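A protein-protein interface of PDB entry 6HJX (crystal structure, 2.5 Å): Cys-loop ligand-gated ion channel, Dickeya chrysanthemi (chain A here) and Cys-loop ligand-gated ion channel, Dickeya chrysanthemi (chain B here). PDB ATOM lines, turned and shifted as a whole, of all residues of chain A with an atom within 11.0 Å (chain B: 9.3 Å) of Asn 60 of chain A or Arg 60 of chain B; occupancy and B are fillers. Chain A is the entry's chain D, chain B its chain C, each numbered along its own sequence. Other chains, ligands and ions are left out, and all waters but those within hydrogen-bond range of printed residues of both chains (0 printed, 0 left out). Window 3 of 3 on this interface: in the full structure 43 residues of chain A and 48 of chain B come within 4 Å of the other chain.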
ATOM      1  N   VAL A  50     -27.577 -40.452  17.432  1.00  0.00           N
ATOM      2  CA  VAL A  50     -27.041 -39.095  17.486  1.00  0.00           C
ATOM      3  C   VAL A  50     -28.169 -38.175  17.928  1.00  0.00           C
ATOM      4  O   VAL A  50     -29.227 -38.135  17.287  1.00  0.00           O
ATOM      5  CB  VAL A  50     -26.473 -38.645  16.132  1.00  0.00           C
ATOM      6  CG1 VAL A  50     -25.675 -37.365  16.300  1.00  0.00           C
ATOM      7  CG2 VAL A  50     -25.616 -39.743  15.516  1.00  0.00           C
ATOM      8  N   ASN A  52     -29.868 -34.463  19.395  1.00  0.00           N
ATOM      9  CA  ASN A  52     -29.914 -33.016  19.573  1.00  0.00           C
ATOM     10  C   ASN A  52     -28.721 -32.298  18.944  1.00  0.00           C
ATOM     11  O   ASN A  52     -28.489 -32.418  17.737  1.00  0.00           O
ATOM     12  CB  ASN A  52     -30.016 -32.699  21.068  1.00  0.00           C
ATOM     13  CG  ASN A  52     -31.292 -33.233  21.690  1.00  0.00           C
ATOM     14  OD1 ASN A  52     -32.364 -33.163  21.089  1.00  0.00           O
ATOM     15  ND2 ASN A  52     -31.183 -33.773  22.897  1.00  0.00           N
ATOM     16  N   THR A  53     -27.959 -31.549  19.748  1.00  0.00           N
ATOM     17  CA  THR A  53     -26.932 -30.664  19.204  1.00  0.00           C
ATOM     18  C   THR A  53     -25.917 -31.400  18.339  1.00  0.00           C
ATOM     19  O   THR A  53     -25.295 -30.780  17.469  1.00  0.00           O
ATOM     20  CB  THR A  53     -26.203 -29.937  20.339  1.00  0.00           C
ATOM     21  OG1 THR A  53     -25.666 -30.895  21.260  1.00  0.00           O
ATOM     22  CG2 THR A  53     -27.149 -29.012  21.079  1.00  0.00           C
ATOM     23  N   GLN A  54     -25.730 -32.703  18.553  1.00  0.00           N
ATOM     24  CA  GLN A  54     -24.766 -33.456  17.762  1.00  0.00           C
ATOM     25  C   GLN A  54     -25.245 -33.706  16.335  1.00  0.00           C
ATOM     26  O   GLN A  54     -24.415 -33.946  15.453  1.00  0.00           O
ATOM     27  CB  GLN A  54     -24.453 -34.780  18.455  1.00  0.00           C
ATOM     28  CG  GLN A  54     -23.897 -34.604  19.856  1.00  0.00           C
ATOM     29  CD  GLN A  54     -22.697 -33.682  19.883  1.00  0.00           C
ATOM     30  OE1 GLN A  54     -21.885 -33.678  18.958  1.00  0.00           O
ATOM     31  NE2 GLN A  54     -22.589 -32.879  20.935  1.00  0.00           N
ATOM     32  N   ILE A  55     -26.557 -33.655  16.088  1.00  0.00           N
ATOM     33  CA  ILE A  55     -27.061 -33.795  14.722  1.00  0.00           C
ATOM     34  C   ILE A  55     -26.398 -32.773  13.810  1.00  0.00           C
ATOM     35  O   ILE A  55     -26.016 -33.081  12.673  1.00  0.00           O
ATOM     36  CB  ILE A  55     -28.595 -33.655  14.702  1.00  0.00           C
ATOM     37  CG1 ILE A  55     -29.247 -34.854  15.393  1.00  0.00           C
ATOM     38  CG2 ILE A  55     -29.110 -33.515  13.270  1.00  0.00           C
ATOM     39  CD1 ILE A  55     -30.732 -34.693  15.636  1.00  0.00           C
ATOM     40  N   GLU A  56     -26.250 -31.537  14.295  1.00  0.00           N
ATOM     41  CA  GLU A  56     -25.725 -30.466  13.456  1.00  0.00           C
ATOM     42  C   GLU A  56     -24.333 -30.789  12.933  1.00  0.00           C
ATOM     43  O   GLU A  56     -23.955 -30.326  11.850  1.00  0.00           O
ATOM     44  CB  GLU A  56     -25.704 -29.156  14.244  1.00  0.00           C
ATOM     45  CG  GLU A  56     -25.324 -27.938  13.418  1.00  0.00           C
ATOM     46  CD  GLU A  56     -26.322 -27.641  12.315  1.00  0.00           C
ATOM     47  OE1 GLU A  56     -27.428 -28.222  12.333  1.00  0.00           O
ATOM     48  OE2 GLU A  56     -25.997 -26.822  11.427  1.00  0.00           O
ATOM     49  N   ARG A  57     -23.558 -31.577  13.678  1.00  0.00           N
ATOM     50  CA  ARG A  57     -22.197 -31.882  13.254  1.00  0.00           C
ATOM     51  C   ARG A  57     -22.176 -32.872  12.096  1.00  0.00           C
ATOM     52  O   ARG A  57     -21.279 -32.810  11.247  1.00  0.00           O
ATOM     53  CB  ARG A  57     -21.393 -32.427  14.435  1.00  0.00           C
ATOM     54  CG  ARG A  57     -21.629 -31.673  15.742  1.00  0.00           C
ATOM     55  CD  ARG A  57     -20.343 -31.528  16.541  1.00  0.00           C
ATOM     56  NE  ARG A  57     -19.600 -32.782  16.618  1.00  0.00           N
ATOM     57  CZ  ARG A  57     -18.333 -32.881  17.010  1.00  0.00           C
ATOM     58  NH1 ARG A  57     -17.656 -31.795  17.361  1.00  0.00           N
ATOM     59  NH2 ARG A  57     -17.740 -34.068  17.042  1.00  0.00           N
ATOM     60  N   TRP A  58     -23.146 -33.788  12.042  1.00  0.00           N
ATOM     61  CA  TRP A  58     -23.230 -34.703  10.908  1.00  0.00           C
ATOM     62  C   TRP A  58     -23.725 -33.989   9.656  1.00  0.00           C
ATOM     63  O   TRP A  58     -23.243 -34.260   8.550  1.00  0.00           O
ATOM     64  CB  TRP A  58     -24.143 -35.879  11.246  1.00  0.00           C
ATOM     65  CG  TRP A  58     -23.506 -36.900  12.142  1.00  0.00           C
ATOM     66  CD1 TRP A  58     -23.354 -36.823  13.495  1.00  0.00           C
ATOM     67  CD2 TRP A  58     -22.942 -38.156  11.747  1.00  0.00           C
ATOM     68  NE1 TRP A  58     -22.726 -37.949  13.967  1.00  0.00           N
ATOM     69  CE2 TRP A  58     -22.462 -38.784  12.913  1.00  0.00           C
ATOM     70  CE3 TRP A  58     -22.792 -38.808  10.520  1.00  0.00           C
ATOM     71  CZ2 TRP A  58     -21.846 -40.033  12.889  1.00  0.00           C
ATOM     72  CZ3 TRP A  58     -22.180 -40.048  10.496  1.00  0.00           C
ATOM     73  CH2 TRP A  58     -21.714 -40.647  11.674  1.00  0.00           C
ATOM     74  N   ILE A  59     -24.687 -33.076   9.805  1.00  0.00           N
ATOM     75  CA  ILE A  59     -25.193 -32.341   8.649  1.00  0.00           C
ATOM     76  C   ILE A  59     -24.087 -31.482   8.050  1.00  0.00           C
ATOM     77  O   ILE A  59     -23.874 -31.472   6.832  1.00  0.00           O
ATOM     78  CB  ILE A  59     -26.422 -31.501   9.043  1.00  0.00           C
ATOM     79  CG1 ILE A  59     -27.542 -32.416   9.547  1.00  0.00           C
ATOM     80  CG2 ILE A  59     -26.903 -30.670   7.858  1.00  0.00           C
ATOM     81  CD1 ILE A  59     -28.706 -31.685  10.169  1.00  0.00           C
ATOM     82  N   ASN A  60     -23.359 -30.751   8.900  1.00  0.00           N
ATOM     83  CA  ASN A  60     -22.234 -29.960   8.420  1.00  0.00           C
ATOM     84  C   ASN A  60     -21.194 -30.815   7.707  1.00  0.00           C
ATOM     85  O   ASN A  60     -20.445 -30.294   6.875  1.00  0.00           O
ATOM     86  CB  ASN A  60     -21.574 -29.214   9.581  1.00  0.00           C
ATOM     87  CG  ASN A  60     -22.490 -28.181  10.210  1.00  0.00           C
ATOM     88  OD1 ASN A  60     -23.367 -27.626   9.550  1.00  0.00           O
ATOM     89  ND2 ASN A  60     -22.286 -27.916  11.493  1.00  0.00           N
ATOM     90  N   ASN A  61     -21.132 -32.110   8.012  1.00  0.00           N
ATOM     91  CA  ASN A  61     -20.179 -33.013   7.383  1.00  0.00           C
ATOM     92  C   ASN A  61     -20.753 -33.747   6.177  1.00  0.00           C
ATOM     93  O   ASN A  61     -20.070 -34.612   5.617  1.00  0.00           O
ATOM     94  CB  ASN A  61     -19.670 -34.031   8.408  1.00  0.00           C
ATOM     95  CG  ASN A  61     -18.326 -33.638   9.001  1.00  0.00           C
ATOM     96  OD1 ASN A  61     -17.303 -34.254   8.705  1.00  0.00           O
ATOM     97  ND2 ASN A  61     -18.323 -32.601   9.831  1.00  0.00           N
ATOM     98  N   GLY A  62     -21.979 -33.432   5.766  1.00  0.00           N
ATOM     99  CA  GLY A  62     -22.544 -33.952   4.532  1.00  0.00           C
ATOM    100  C   GLY A  62     -23.785 -34.803   4.693  1.00  0.00           C
ATOM    101  O   GLY A  62     -24.470 -35.055   3.689  1.00  0.00           O
ATOM    102  N   LEU A  63     -24.120 -35.266   5.896  1.00  0.00           N
ATOM    103  CA  LEU A  63     -25.301 -36.105   6.058  1.00  0.00           C
ATOM    104  C   LEU A  63     -26.538 -35.357   5.583  1.00  0.00           C
ATOM    105  O   LEU A  63     -26.856 -34.276   6.088  1.00  0.00           O
ATOM    106  CB  LEU A  63     -25.471 -36.532   7.514  1.00  0.00           C
ATOM    107  CG  LEU A  63     -26.695 -37.420   7.777  1.00  0.00           C
ATOM    108  CD1 LEU A  63     -26.552 -38.766   7.081  1.00  0.00           C
ATOM    109  CD2 LEU A  63     -26.924 -37.612   9.266  1.00  0.00           C
ATOM    110  N   TRP A  64     -27.233 -35.945   4.618  1.00  0.00           N
ATOM    111  CA  TRP A  64     -28.435 -35.352   4.048  1.00  0.00           C
ATOM    112  C   TRP A  64     -29.598 -35.545   5.014  1.00  0.00           C
ATOM    113  O   TRP A  64     -29.925 -36.679   5.379  1.00  0.00           O
ATOM    114  CB  TRP A  64     -28.721 -35.995   2.691  1.00  0.00           C
ATOM    115  CG  TRP A  64     -29.914 -35.445   1.983  1.00  0.00           C
ATOM    116  CD1 TRP A  64     -30.047 -34.196   1.449  1.00  0.00           C
ATOM    117  CD2 TRP A  64     -31.141 -36.132   1.712  1.00  0.00           C
ATOM    118  NE1 TRP A  64     -31.284 -34.061   0.869  1.00  0.00           N
ATOM    119  CE2 TRP A  64     -31.974 -35.235   1.015  1.00  0.00           C
ATOM    120  CE3 TRP A  64     -31.616 -37.415   1.992  1.00  0.00           C
ATOM    121  CZ2 TRP A  64     -33.258 -35.582   0.596  1.00  0.00           C
ATOM    122  CZ3 TRP A  64     -32.889 -37.758   1.576  1.00  0.00           C
ATOM    123  CH2 TRP A  64     -33.696 -36.845   0.886  1.00  0.00           C
ATOM    124  N   VAL A  65     -30.203 -34.445   5.450  1.00  0.00           N
ATOM    125  CA  VAL A  65     -31.361 -34.492   6.341  1.00  0.00           C
ATOM    126  C   VAL A  65     -32.365 -33.445   5.870  1.00  0.00           C
ATOM    127  O   VAL A  65     -32.304 -32.288   6.314  1.00  0.00           O
ATOM    128  CB  VAL A  65     -30.957 -34.254   7.805  1.00  0.00           C
ATOM    129  CG1 VAL A  65     -32.180 -34.316   8.717  1.00  0.00           C
ATOM    130  CG2 VAL A  65     -29.919 -35.277   8.247  1.00  0.00           C
ATOM    131  N   LEU A  84     -31.131 -38.826  15.504  1.00  0.00           N
ATOM    132  CA  LEU A  84     -30.945 -39.638  14.313  1.00  0.00           C
ATOM    133  C   LEU A  84     -30.527 -41.040  14.735  1.00  0.00           C
ATOM    134  O   LEU A  84     -29.861 -41.223  15.758  1.00  0.00           O
ATOM    135  CB  LEU A  84     -29.877 -39.047  13.389  1.00  0.00           C
ATOM    136  CG  LEU A  84     -30.185 -37.720  12.698  1.00  0.00           C
ATOM    137  CD1 LEU A  84     -28.935 -37.205  12.002  1.00  0.00           C
ATOM    138  CD2 LEU A  84     -31.326 -37.875  11.702  1.00  0.00           C
ATOM    139  N   LEU A  86     -28.567 -43.950  12.664  1.00  0.00           N
ATOM    140  CA  LEU A  86     -27.879 -44.216  11.405  1.00  0.00           C
ATOM    141  C   LEU A  86     -27.476 -45.686  11.365  1.00  0.00           C
ATOM    142  O   LEU A  86     -26.628 -46.128  12.147  1.00  0.00           O
ATOM    143  CB  LEU A  86     -26.665 -43.302  11.257  1.00  0.00           C
ATOM    144  CG  LEU A  86     -26.950 -41.807  11.433  1.00  0.00           C
ATOM    145  CD1 LEU A  86     -25.676 -40.997  11.244  1.00  0.00           C
ATOM    146  CD2 LEU A  86     -28.043 -41.329  10.475  1.00  0.00           C
ATOM    147  N   VAL B  53     -29.595 -25.569  -0.223  1.00  0.00           N
ATOM    148  CA  VAL B  53     -28.963 -25.371   1.078  1.00  0.00           C
ATOM    149  C   VAL B  53     -30.045 -24.904   2.044  1.00  0.00           C
ATOM    150  O   VAL B  53     -30.654 -23.850   1.829  1.00  0.00           O
ATOM    151  CB  VAL B  53     -27.818 -24.345   1.014  1.00  0.00           C
ATOM    152  CG1 VAL B  53     -27.141 -24.210   2.370  1.00  0.00           C
ATOM    153  CG2 VAL B  53     -26.803 -24.736  -0.054  1.00  0.00           C
ATOM    154  N   GLU B  54     -30.276 -25.673   3.105  1.00  0.00           N
ATOM    155  CA  GLU B  54     -31.383 -25.421   4.019  1.00  0.00           C
ATOM    156  C   GLU B  54     -30.892 -24.892   5.361  1.00  0.00           C
ATOM    157  O   GLU B  54     -29.882 -25.360   5.898  1.00  0.00           O
ATOM    158  CB  GLU B  54     -32.206 -26.695   4.242  1.00  0.00           C
ATOM    159  CG  GLU B  54     -33.026 -27.130   3.038  1.00  0.00           C
ATOM    160  CD  GLU B  54     -33.752 -28.441   3.265  1.00  0.00           C
ATOM    161  OE1 GLU B  54     -33.149 -29.366   3.847  1.00  0.00           O
ATOM    162  OE2 GLU B  54     -34.929 -28.546   2.864  1.00  0.00           O
ATOM    163  N   ASN B  55     -31.613 -23.896   5.886  1.00  0.00           N
ATOM    164  CA  ASN B  55     -31.527 -23.471   7.280  1.00  0.00           C
ATOM    165  C   ASN B  55     -30.101 -23.204   7.760  1.00  0.00           C
ATOM    166  O   ASN B  55     -29.455 -22.263   7.287  1.00  0.00           O
ATOM    167  CB  ASN B  55     -32.218 -24.521   8.160  1.00  0.00           C
ATOM    168  CG  ASN B  55     -33.721 -24.577   7.926  1.00  0.00           C
ATOM    169  OD1 ASN B  55     -34.381 -23.542   7.852  1.00  0.00           O
ATOM    170  ND2 ASN B  55     -34.266 -25.782   7.797  1.00  0.00           N
ATOM    171  N   THR B  56     -29.605 -23.999   8.714  1.00  0.00           N
ATOM    172  CA  THR B  56     -28.311 -23.701   9.328  1.00  0.00           C
ATOM    173  C   THR B  56     -27.195 -23.670   8.294  1.00  0.00           C
ATOM    174  O   THR B  56     -26.275 -22.849   8.388  1.00  0.00           O
ATOM    175  CB  THR B  56     -27.981 -24.729  10.414  1.00  0.00           C
ATOM    176  OG1 THR B  56     -28.025 -26.051   9.861  1.00  0.00           O
ATOM    177  CG2 THR B  56     -28.957 -24.633  11.564  1.00  0.00           C
ATOM    178  N   GLN B  57     -27.250 -24.561   7.302  1.00  0.00           N
ATOM    179  CA  GLN B  57     -26.188 -24.623   6.305  1.00  0.00           C
ATOM    180  C   GLN B  57     -26.030 -23.303   5.564  1.00  0.00           C
ATOM    181  O   GLN B  57     -24.942 -23.005   5.060  1.00  0.00           O
ATOM    182  CB  GLN B  57     -26.464 -25.756   5.318  1.00  0.00           C
ATOM    183  CG  GLN B  57     -26.565 -27.117   5.978  1.00  0.00           C
ATOM    184  CD  GLN B  57     -25.314 -27.475   6.755  1.00  0.00           C
ATOM    185  OE1 GLN B  57     -24.256 -27.717   6.174  1.00  0.00           O
ATOM    186  NE2 GLN B  57     -25.427 -27.499   8.078  1.00  0.00           N
ATOM    187  N   ILE B  58     -27.095 -22.500   5.483  1.00  0.00           N
ATOM    188  CA  ILE B  58     -26.989 -21.204   4.821  1.00  0.00           C
ATOM    189  C   ILE B  58     -25.897 -20.367   5.475  1.00  0.00           C
ATOM    190  O   ILE B  58     -25.146 -19.656   4.797  1.00  0.00           O
ATOM    191  CB  ILE B  58     -28.349 -20.478   4.838  1.00  0.00           C
ATOM    192  CG1 ILE B  58     -29.375 -21.252   4.006  1.00  0.00           C
ATOM    193  CG2 ILE B  58     -28.208 -19.055   4.305  1.00  0.00           C
ATOM    194  CD1 ILE B  58     -30.793 -20.725   4.121  1.00  0.00           C
ATOM    195  N   GLU B  59     -25.785 -20.450   6.803  1.00  0.00           N
ATOM    196  CA  GLU B  59     -24.795 -19.650   7.518  1.00  0.00           C
ATOM    197  C   GLU B  59     -23.377 -20.006   7.086  1.00  0.00           C
ATOM    198  O   GLU B  59     -22.505 -19.132   7.007  1.00  0.00           O
ATOM    199  CB  GLU B  59     -24.963 -19.847   9.026  1.00  0.00           C
ATOM    200  CG  GLU B  59     -24.506 -18.665   9.853  1.00  0.00           C
ATOM    201  CD  GLU B  59     -25.346 -17.430   9.599  1.00  0.00           C
ATOM    202  OE1 GLU B  59     -26.538 -17.582   9.259  1.00  0.00           O
ATOM    203  OE2 GLU B  59     -24.812 -16.307   9.734  1.00  0.00           O
ATOM    204  N   ARG B  60     -23.126 -21.284   6.795  1.00  0.00           N
ATOM    205  CA  ARG B  60     -21.794 -21.694   6.365  1.00  0.00           C
ATOM    206  C   ARG B  60     -21.420 -21.041   5.041  1.00  0.00           C
ATOM    207  O   ARG B  60     -20.253 -20.698   4.817  1.00  0.00           O
ATOM    208  CB  ARG B  60     -21.725 -23.215   6.240  1.00  0.00           C
ATOM    209  CG  ARG B  60     -22.198 -23.964   7.476  1.00  0.00           C
ATOM    210  CD  ARG B  60     -22.023 -25.464   7.298  1.00  0.00           C
ATOM    211  NE  ARG B  60     -20.649 -25.892   7.546  1.00  0.00           N
ATOM    212  CZ  ARG B  60     -20.123 -27.029   7.099  1.00  0.00           C
ATOM    213  NH1 ARG B  60     -20.848 -27.861   6.362  1.00  0.00           N
ATOM    214  NH2 ARG B  60     -18.863 -27.333   7.381  1.00  0.00           N
ATOM    215  N   TRP B  61     -22.399 -20.859   4.151  1.00  0.00           N
ATOM    216  CA  TRP B  61     -22.115 -20.270   2.846  1.00  0.00           C
ATOM    217  C   TRP B  61     -21.869 -18.771   2.958  1.00  0.00           C
ATOM    218  O   TRP B  61     -21.042 -18.218   2.225  1.00  0.00           O
ATOM    219  CB  TRP B  61     -23.266 -20.554   1.884  1.00  0.00           C
ATOM    220  CG  TRP B  61     -23.258 -21.947   1.351  1.00  0.00           C
ATOM    221  CD1 TRP B  61     -23.711 -23.071   1.981  1.00  0.00           C
ATOM    222  CD2 TRP B  61     -22.774 -22.372   0.074  1.00  0.00           C
ATOM    223  NE1 TRP B  61     -23.537 -24.167   1.174  1.00  0.00           N
ATOM    224  CE2 TRP B  61     -22.963 -23.764  -0.003  1.00  0.00           C
ATOM    225  CE3 TRP B  61     -22.200 -21.706  -1.014  1.00  0.00           C
ATOM    226  CZ2 TRP B  61     -22.598 -24.505  -1.125  1.00  0.00           C
ATOM    227  CZ3 TRP B  61     -21.837 -22.444  -2.126  1.00  0.00           C
ATOM    228  CH2 TRP B  61     -22.038 -23.828  -2.173  1.00  0.00           C
ATOM    229  N   ILE B  62     -22.577 -18.098   3.865  1.00  0.00           N
ATOM    230  CA  ILE B  62     -22.343 -16.672   4.072  1.00  0.00           C
ATOM    231  C   ILE B  62     -20.937 -16.440   4.619  1.00  0.00           C
ATOM    232  O   ILE B  62     -20.271 -15.462   4.256  1.00  0.00           O
ATOM    233  CB  ILE B  62     -23.425 -16.085   4.998  1.00  0.00           C
ATOM    234  CG1 ILE B  62     -24.805 -16.226   4.346  1.00  0.00           C
ATOM    235  CG2 ILE B  62     -23.141 -14.618   5.303  1.00  0.00           C
ATOM    236  CD1 ILE B  62     -25.962 -16.082   5.311  1.00  0.00           C
ATOM    237  N   ASN B  63     -20.460 -17.334   5.493  1.00  0.00           N
ATOM    238  CA  ASN B  63     -19.096 -17.219   5.999  1.00  0.00           C
ATOM    239  C   ASN B  63     -18.071 -17.370   4.883  1.00  0.00           C
ATOM    240  O   ASN B  63     -16.986 -16.782   4.953  1.00  0.00           O
ATOM    241  CB  ASN B  63     -18.841 -18.270   7.083  1.00  0.00           C
ATOM    242  CG  ASN B  63     -19.730 -18.087   8.294  1.00  0.00           C
ATOM    243  OD1 ASN B  63     -20.317 -17.025   8.498  1.00  0.00           O
ATOM    244  ND2 ASN B  63     -19.830 -19.126   9.112  1.00  0.00           N
ATOM    245  N   ASN B  64     -18.393 -18.153   3.854  1.00  0.00           N
ATOM    246  CA  ASN B  64     -17.503 -18.349   2.716  1.00  0.00           C
ATOM    247  C   ASN B  64     -17.579 -17.220   1.698  1.00  0.00           C
ATOM    248  O   ASN B  64     -16.930 -17.312   0.652  1.00  0.00           O
ATOM    249  CB  ASN B  64     -17.822 -19.673   2.025  1.00  0.00           C
ATOM    250  CG  ASN B  64     -16.945 -20.804   2.506  1.00  0.00           C
ATOM    251  OD1 ASN B  64     -15.996 -21.197   1.826  1.00  0.00           O
ATOM    252  ND2 ASN B  64     -17.251 -21.332   3.687  1.00  0.00           N
ATOM    253  N   GLY B  65     -18.353 -16.171   1.967  1.00  0.00           N
ATOM    254  CA  GLY B  65     -18.418 -15.018   1.091  1.00  0.00           C
ATOM    255  C   GLY B  65     -19.675 -14.908   0.255  1.00  0.00           C
ATOM    256  O   GLY B  65     -19.797 -13.944  -0.513  1.00  0.00           O
ATOM    257  N   LEU B  66     -20.612 -15.849   0.365  1.00  0.00           N
ATOM    258  CA  LEU B  66     -21.849 -15.759  -0.402  1.00  0.00           C
ATOM    259  C   LEU B  66     -22.685 -14.584   0.090  1.00  0.00           C
ATOM    260  O   LEU B  66     -22.984 -14.474   1.282  1.00  0.00           O
ATOM    261  CB  LEU B  66     -22.656 -17.051  -0.292  1.00  0.00           C
ATOM    262  CG  LEU B  66     -23.967 -17.058  -1.092  1.00  0.00           C
ATOM    263  CD1 LEU B  66     -23.695 -17.085  -2.590  1.00  0.00           C
ATOM    264  CD2 LEU B  66     -24.856 -18.223  -0.686  1.00  0.00           C
ATOM    265  N   VAL B  68     -25.863 -12.715   0.824  1.00  0.00           N
ATOM    266  CA  VAL B  68     -27.280 -12.969   1.072  1.00  0.00           C
ATOM    267  C   VAL B  68     -27.837 -11.795   1.868  1.00  0.00           C
ATOM    268  O   VAL B  68     -27.768 -11.805   3.104  1.00  0.00           O
ATOM    269  CB  VAL B  68     -27.494 -14.293   1.821  1.00  0.00           C
ATOM    270  CG1 VAL B  68     -28.989 -14.590   1.960  1.00  0.00           C
ATOM    271  CG2 VAL B  68     -26.786 -15.424   1.102  1.00  0.00           C
ATOM    272  N   LEU B  87     -31.915 -21.761   0.332  1.00  0.00           N
ATOM    273  CA  LEU B  87     -31.277 -21.149  -0.823  1.00  0.00           C
ATOM    274  C   LEU B  87     -31.198 -22.172  -1.947  1.00  0.00           C
ATOM    275  O   LEU B  87     -31.003 -23.367  -1.696  1.00  0.00           O
ATOM    276  CB  LEU B  87     -29.865 -20.652  -0.496  1.00  0.00           C
ATOM    277  CG  LEU B  87     -29.711 -19.276   0.151  1.00  0.00           C
ATOM    278  CD1 LEU B  87     -28.250 -19.045   0.516  1.00  0.00           C
ATOM    279  CD2 LEU B  87     -30.207 -18.177  -0.773  1.00  0.00           C
ATOM    280  N   LEU B  89     -28.983 -22.500  -5.470  1.00  0.00           N
ATOM    281  CA  LEU B  89     -27.865 -21.940  -6.220  1.00  0.00           C
ATOM    282  C   LEU B  89     -27.747 -22.658  -7.557  1.00  0.00           C
ATOM    283  O   LEU B  89     -27.533 -23.874  -7.597  1.00  0.00           O
ATOM    284  CB  LEU B  89     -26.563 -22.071  -5.431  1.00  0.00           C
ATOM    285  CG  LEU B  89     -26.604 -21.543  -3.996  1.00  0.00           C
ATOM    286  CD1 LEU B  89     -25.314 -21.895  -3.264  1.00  0.00           C
ATOM    287  CD2 LEU B  89     -26.842 -20.041  -3.986  1.00  0.00           C
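The side-chain hydroxyl (OG1) of Thr 56 of chain B sits at hydrogen-bond distance from the side-chain carboxylate (OE2) of Glu 56 of chain A, at 2.7 Å. The side-chain amide nitrogen (NE2) of Gln 57 of chain B sits at hydrogen-bond distance from the side-chain carboxylate (OE2) of Glu 56 of chain A. The side-chain amide nitrogen of Gln 57 of chain B sits at hydrogen-bond distance from the side-chain amide oxygen of Asn 60 of chain A, 2.5 Å away. O of Asn 60 of chain A lies within hydrogen-bond range of NH1 of Arg 60 of chain B (2.5 Å).
The side-chain hydroxyl of Thr 56 of chain B lies within hydrogen-bond range of the side-chain amide nitrogen of Gln 57 of chain B (3.5 Å). NH1 of Arg 60 of chain B sits close to OE1 of Gln 57 of chain B, at 3.4 Å. O of Arg 60 of chain B lies within hydrogen-bond range of ND2 of Asn 64 of chain B. O of Glu 56 of chain A sits at hydrogen-bond distance from ND2 of Asn 60 of chain A (3.0 Å).
CG2 of Ile 59 of chain A touches NE2 of Gln 57 of chain B, at 3.5 Å. Glu 54 of chain B touches Val 65 of chain A.
Gln 54 of chain A touches none of the printed residues of chain B. Of the printed residues of chain B, Glu 56 of chain A touches Thr 56 (2.7 Å) and Gln 57 (3.5 Å). Of the printed residues of chain B, Asn 60 of chain A touches Gln 57 and Arg 60. Of the printed residues of chain B, Val 65 of chain A touches Glu 54 (3.9 Å). Of the printed residues of chain A, Thr 56 of chain B touches Glu 56 (2.7 Å). Printed residues of chain A within 4 Å of Gln 57 of chain B: Glu 56 (3.5 Å), Ile 59 (3.5 Å) and Asn 60 (2.5 Å). No residue of chain A comes within 4 Å of Glu 59 of chain B. Arg 60 of chain B touches just one residue of chain A: Asn 60 (2.5 Å). Trp 61 of chain B touches none of the printed residues of chain A. No residue of chain A comes within 4 Å of Asn 64 of chain B. The nearest residue of chain A that does not touch Arg 60 of chain B is Asn 61 of chain A (4.6 Å).
Printed residues of chain B that touch a printed residue of chain A: Glu 54, Thr 56, Gln 57 and Arg 60. Along chain A the printed residues that touch a printed residue of chain B span positions 56 to 65. Among the printed residues, 6 pairs touch across the chains. Among the printed residues, no Asp or Glu carboxylate lies within 4 Å of a Lys or Arg side-chain nitrogen of the other chain.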
